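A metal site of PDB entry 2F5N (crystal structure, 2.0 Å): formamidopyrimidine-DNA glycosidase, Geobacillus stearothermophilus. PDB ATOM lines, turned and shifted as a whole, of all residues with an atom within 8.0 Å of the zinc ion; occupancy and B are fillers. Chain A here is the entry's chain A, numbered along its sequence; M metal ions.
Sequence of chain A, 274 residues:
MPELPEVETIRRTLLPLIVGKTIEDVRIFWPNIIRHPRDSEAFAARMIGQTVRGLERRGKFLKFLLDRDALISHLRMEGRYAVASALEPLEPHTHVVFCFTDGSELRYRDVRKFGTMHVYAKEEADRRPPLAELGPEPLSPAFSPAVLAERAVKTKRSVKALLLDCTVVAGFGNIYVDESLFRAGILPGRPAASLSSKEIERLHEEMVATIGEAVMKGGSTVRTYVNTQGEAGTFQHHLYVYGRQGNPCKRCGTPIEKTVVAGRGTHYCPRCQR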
ATOM      1  N   PHE A 182      21.505 -22.875   7.900  1.00  0.00           N
ATOM      2  CA  PHE A 182      22.433 -21.785   8.345  1.00  0.00           C
ATOM      3  C   PHE A 182      23.828 -22.070   7.763  1.00  0.00           C
ATOM      4  O   PHE A 182      24.441 -21.200   7.183  1.00  0.00           O
ATOM      5  CB  PHE A 182      22.552 -21.789   9.846  1.00  0.00           C
ATOM      6  CG  PHE A 182      23.690 -20.987  10.308  1.00  0.00           C
ATOM      7  CD1 PHE A 182      23.531 -19.596  10.460  1.00  0.00           C
ATOM      8  CD2 PHE A 182      24.955 -21.590  10.502  1.00  0.00           C
ATOM      9  CE1 PHE A 182      24.620 -18.775  10.824  1.00  0.00           C
ATOM     10  CE2 PHE A 182      26.032 -20.780  10.860  1.00  0.00           C
ATOM     11  CZ  PHE A 182      25.845 -19.368  11.024  1.00  0.00           C
ATOM     12  N   TYR A 240      24.594 -23.664  16.004  1.00  0.00           N
ATOM     13  CA  TYR A 240      24.667 -22.294  15.469  1.00  0.00           C
ATOM     14  C   TYR A 240      23.402 -21.426  15.688  1.00  0.00           C
ATOM     15  O   TYR A 240      23.460 -20.210  16.081  1.00  0.00           O
ATOM     16  CB  TYR A 240      24.983 -22.328  13.955  1.00  0.00           C
ATOM     17  CG  TYR A 240      26.388 -22.779  13.654  1.00  0.00           C
ATOM     18  CD1 TYR A 240      26.630 -24.052  13.170  1.00  0.00           C
ATOM     19  CD2 TYR A 240      27.491 -21.932  13.886  1.00  0.00           C
ATOM     20  CE1 TYR A 240      27.887 -24.524  12.925  1.00  0.00           C
ATOM     21  CE2 TYR A 240      28.799 -22.390  13.668  1.00  0.00           C
ATOM     22  CZ  TYR A 240      28.982 -23.700  13.184  1.00  0.00           C
ATOM     23  OH  TYR A 240      30.237 -24.270  13.003  1.00  0.00           O
ATOM     24  N   VAL A 241      22.260 -22.036  15.431  1.00  0.00           N
ATOM     25  CA  VAL A 241      20.992 -21.302  15.496  1.00  0.00           C
ATOM     26  C   VAL A 241      19.847 -21.955  16.299  1.00  0.00           C
ATOM     27  O   VAL A 241      19.102 -21.265  16.997  1.00  0.00           O
ATOM     28  CB  VAL A 241      20.440 -21.048  14.063  1.00  0.00           C
ATOM     29  CG1 VAL A 241      21.438 -20.256  13.251  1.00  0.00           C
ATOM     30  CG2 VAL A 241      20.144 -22.430  13.335  1.00  0.00           C
ATOM     31  N   PRO A 248      23.492 -13.981  20.107  1.00  0.00           N
ATOM     32  CA  PRO A 248      24.249 -13.579  18.917  1.00  0.00           C
ATOM     33  C   PRO A 248      24.646 -14.803  18.100  1.00  0.00           C
ATOM     34  O   PRO A 248      24.994 -15.876  18.642  1.00  0.00           O
ATOM     35  CB  PRO A 248      25.476 -12.866  19.489  1.00  0.00           C
ATOM     36  CG  PRO A 248      25.573 -13.408  20.929  1.00  0.00           C
ATOM     37  CD  PRO A 248      24.154 -13.588  21.364  1.00  0.00           C
ATOM     38  N   CYS A 249      24.643 -14.605  16.792  1.00  0.00           N
ATOM     39  CA  CYS A 249      25.081 -15.595  15.852  1.00  0.00           C
ATOM     40  C   CYS A 249      26.573 -15.801  16.160  1.00  0.00           C
ATOM     41  O   CYS A 249      27.355 -14.853  16.368  1.00  0.00           O
ATOM     42  CB  CYS A 249      24.936 -15.065  14.408  1.00  0.00           C
ATOM     43  SG  CYS A 249      25.735 -16.141  13.178  1.00  0.00           S
ATOM     44  N   LYS A 250      26.958 -17.050  16.174  1.00  0.00           N
ATOM     45  CA  LYS A 250      28.338 -17.472  16.434  1.00  0.00           C
ATOM     46  C   LYS A 250      29.307 -17.078  15.362  1.00  0.00           C
ATOM     47  O   LYS A 250      30.520 -16.992  15.592  1.00  0.00           O
ATOM     48  CB  LYS A 250      28.375 -19.012  16.613  1.00  0.00           C
ATOM     49  CG  LYS A 250      27.618 -19.345  17.888  1.00  0.00           C
ATOM     50  CD  LYS A 250      27.605 -20.815  18.214  1.00  0.00           C
ATOM     51  CE  LYS A 250      27.070 -21.001  19.672  1.00  0.00           C
ATOM     52  NZ  LYS A 250      27.336 -22.369  20.194  1.00  0.00           N
ATOM     53  N   ARG A 251      28.774 -16.845  14.174  1.00  0.00           N
ATOM     54  CA  ARG A 251      29.637 -16.448  13.080  1.00  0.00           C
ATOM     55  C   ARG A 251      29.719 -14.908  12.925  1.00  0.00           C
ATOM     56  O   ARG A 251      30.770 -14.358  12.565  1.00  0.00           O
ATOM     57  CB  ARG A 251      29.093 -17.036  11.747  1.00  0.00           C
ATOM     58  CG  ARG A 251      29.679 -16.517  10.499  1.00  0.00           C
ATOM     59  CD  ARG A 251      30.050 -17.683   9.684  1.00  0.00           C
ATOM     60  NE  ARG A 251      29.007 -18.085   8.796  1.00  0.00           N
ATOM     61  CZ  ARG A 251      28.721 -19.353   8.489  1.00  0.00           C
ATOM     62  NH1 ARG A 251      27.740 -19.598   7.628  1.00  0.00           N
ATOM     63  NH2 ARG A 251      29.367 -20.362   9.095  1.00  0.00           N
ATOM     64  N   CYS A 252      28.605 -14.201  13.123  1.00  0.00           N
ATOM     65  CA  CYS A 252      28.684 -12.739  12.872  1.00  0.00           C
ATOM     66  C   CYS A 252      28.198 -11.852  13.995  1.00  0.00           C
ATOM     67  O   CYS A 252      28.237 -10.620  13.890  1.00  0.00           O
ATOM     68  CB  CYS A 252      27.880 -12.432  11.582  1.00  0.00           C
ATOM     69  SG  CYS A 252      26.016 -12.504  11.910  1.00  0.00           S
ATOM     70  N   GLY A 253      27.684 -12.416  15.070  1.00  0.00           N
ATOM     71  CA  GLY A 253      27.219 -11.553  16.149  1.00  0.00           C
ATOM     72  C   GLY A 253      25.785 -11.011  16.046  1.00  0.00           C
ATOM     73  O   GLY A 253      25.249 -10.520  17.050  1.00  0.00           O
ATOM     74  N   THR A 254      25.173 -11.024  14.857  1.00  0.00           N
ATOM     75  CA  THR A 254      23.773 -10.593  14.688  1.00  0.00           C
ATOM     76  C   THR A 254      22.840 -11.517  15.521  1.00  0.00           C
ATOM     77  O   THR A 254      23.013 -12.776  15.540  1.00  0.00           O
ATOM     78  CB  THR A 254      23.368 -10.762  13.237  1.00  0.00           C
ATOM     79  OG1 THR A 254      24.158  -9.926  12.397  1.00  0.00           O
ATOM     80  CG2 THR A 254      21.918 -10.478  13.084  1.00  0.00           C
ATOM     81  N   PRO A 255      21.830 -10.947  16.222  1.00  0.00           N
ATOM     82  CA  PRO A 255      20.980 -11.880  16.981  1.00  0.00           C
ATOM     83  C   PRO A 255      20.188 -12.901  16.094  1.00  0.00           C
ATOM     84  O   PRO A 255      19.554 -12.529  15.064  1.00  0.00           O
ATOM     85  CB  PRO A 255      19.997 -10.968  17.711  1.00  0.00           C
ATOM     86  CG  PRO A 255      20.785  -9.532  17.784  1.00  0.00           C
ATOM     87  CD  PRO A 255      21.436  -9.520  16.416  1.00  0.00           C
ATOM     88  N   ILE A 256      20.213 -14.168  16.521  1.00  0.00           N
ATOM     89  CA  ILE A 256      19.459 -15.209  15.791  1.00  0.00           C
ATOM     90  C   ILE A 256      17.952 -14.923  15.919  1.00  0.00           C
ATOM     91  O   ILE A 256      17.481 -14.529  16.973  1.00  0.00           O
ATOM     92  CB  ILE A 256      19.741 -16.574  16.416  1.00  0.00           C
ATOM     93  CG1 ILE A 256      21.274 -16.873  16.279  1.00  0.00           C
ATOM     94  CG2 ILE A 256      18.890 -17.668  15.775  1.00  0.00           C
ATOM     95  CD1 ILE A 256      21.794 -16.664  14.737  1.00  0.00           C
ATOM     96  N   TYR A 268      17.233 -18.804  12.521  1.00  0.00           N
ATOM     97  CA  TYR A 268      18.142 -18.490  11.419  1.00  0.00           C
ATOM     98  C   TYR A 268      18.878 -17.122  11.695  1.00  0.00           C
ATOM     99  O   TYR A 268      18.471 -16.323  12.547  1.00  0.00           O
ATOM    100  CB  TYR A 268      17.333 -18.429  10.085  1.00  0.00           C
ATOM    101  CG  TYR A 268      16.283 -17.343  10.064  1.00  0.00           C
ATOM    102  CD1 TYR A 268      16.626 -16.025   9.760  1.00  0.00           C
ATOM    103  CD2 TYR A 268      14.991 -17.591  10.470  1.00  0.00           C
ATOM    104  CE1 TYR A 268      15.708 -14.986   9.885  1.00  0.00           C
ATOM    105  CE2 TYR A 268      14.038 -16.560  10.594  1.00  0.00           C
ATOM    106  CZ  TYR A 268      14.404 -15.264  10.308  1.00  0.00           C
ATOM    107  OH  TYR A 268      13.505 -14.225  10.481  1.00  0.00           O
ATOM    108  N   CYS A 269      20.000 -16.941  11.030  1.00  0.00           N
ATOM    109  CA  CYS A 269      20.715 -15.676  11.107  1.00  0.00           C
ATOM    110  C   CYS A 269      20.251 -14.824   9.894  1.00  0.00           C
ATOM    111  O   CYS A 269      20.441 -15.210   8.735  1.00  0.00           O
ATOM    112  CB  CYS A 269      22.225 -15.929  11.045  1.00  0.00           C
ATOM    113  SG  CYS A 269      23.047 -14.317  10.867  1.00  0.00           S
ATOM    114  N   PRO A 270      19.552 -13.716  10.142  1.00  0.00           N
ATOM    115  CA  PRO A 270      19.083 -12.880   9.006  1.00  0.00           C
ATOM    116  C   PRO A 270      20.161 -12.253   8.199  1.00  0.00           C
ATOM    117  O   PRO A 270      19.939 -11.868   7.079  1.00  0.00           O
ATOM    118  CB  PRO A 270      18.219 -11.805   9.659  1.00  0.00           C
ATOM    119  CG  PRO A 270      18.741 -11.686  11.055  1.00  0.00           C
ATOM    120  CD  PRO A 270      19.133 -13.167  11.456  1.00  0.00           C
ATOM    121  N   ARG A 271      21.353 -12.095   8.755  1.00  0.00           N
ATOM    122  CA  ARG A 271      22.390 -11.503   7.961  1.00  0.00           C
ATOM    123  C   ARG A 271      23.072 -12.512   7.064  1.00  0.00           C
ATOM    124  O   ARG A 271      23.379 -12.224   5.914  1.00  0.00           O
ATOM    125  CB  ARG A 271      23.426 -10.853   8.877  1.00  0.00           C
ATOM    126  CG  ARG A 271      24.682 -10.400   8.177  1.00  0.00           C
ATOM    127  CD  ARG A 271      25.805  -9.947   9.201  1.00  0.00           C
ATOM    128  NE  ARG A 271      26.967  -9.537   8.426  1.00  0.00           N
ATOM    129  CZ  ARG A 271      27.967  -8.792   8.894  1.00  0.00           C
ATOM    130  NH1 ARG A 271      28.936  -8.420   8.057  1.00  0.00           N
ATOM    131  NH2 ARG A 271      28.025  -8.491  10.170  1.00  0.00           N
ATOM    132  N   CYS A 272      23.334 -13.713   7.600  1.00  0.00           N
ATOM    133  CA  CYS A 272      24.064 -14.716   6.856  1.00  0.00           C
ATOM    134  C   CYS A 272      23.263 -15.672   5.961  1.00  0.00           C
ATOM    135  O   CYS A 272      23.840 -16.291   5.084  1.00  0.00           O
ATOM    136  CB  CYS A 272      24.880 -15.513   7.805  1.00  0.00           C
ATOM    137  SG  CYS A 272      26.254 -14.420   8.647  1.00  0.00           S
ATOM    138  N   GLN A 273      21.955 -15.788   6.184  1.00  0.00           N
ATOM    139  CA  GLN A 273      21.196 -16.675   5.343  1.00  0.00           C
ATOM    140  C   GLN A 273      20.412 -15.830   4.340  1.00  0.00           C
ATOM    141  O   GLN A 273      19.766 -14.900   4.774  1.00  0.00           O
ATOM    142  CB  GLN A 273      20.229 -17.488   6.242  1.00  0.00           C
ATOM    143  CG  GLN A 273      21.029 -18.564   6.974  1.00  0.00           C
ATOM    144  CD  GLN A 273      20.229 -19.285   8.013  1.00  0.00           C
ATOM    145  OE1 GLN A 273      20.401 -19.037   9.210  1.00  0.00           O
ATOM    146  NE2 GLN A 273      19.359 -20.238   7.557  1.00  0.00           N
HETATM  147 ZN    ZN M   1      25.289 -14.639  11.443  1.00  0.00          ZN
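The side-chain sulfur (SG) of Cys 252 sits close to the side-chain sulfur (SG) of Cys 272, at 3.8 Å.
SG of Cys 252 lies close to OG1 of Thr 254 (3.2 Å).
The side-chain sulfur of Cys 249 sits close to the backbone NH of Arg 251 (3.3 Å).
The backbone NH of Cys 249 is in hydrogen-bond range of the backbone carbonyl oxygen of Thr 254 (2.8 Å).
The backbone NH (N) of Cys 272 lies close to the side-chain sulfur (SG) of Cys 269.
N of Arg 271 lies close to SG of Cys 269 (3.5 Å).
N of Cys 269 lies within hydrogen-bond range of OE1 of Gln 273.
The nearest printed residue that does not touch the zinc ion is Phe 182 (4.2 Å).
The zinc ion is bound by the side-chain sulfur (SG) of Cys 252 (2.3 Å).
The zinc ion is bound by SG of Cys 249 (2.3 Å).
The side-chain sulfur (SG) of Cys 269 is bound to the zinc ion, 2.3 Å away.
The zinc ion has three donor atoms within binding distance.
Slightly farther from the zinc ion lies SG of Cys 272 (3.0 Å).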
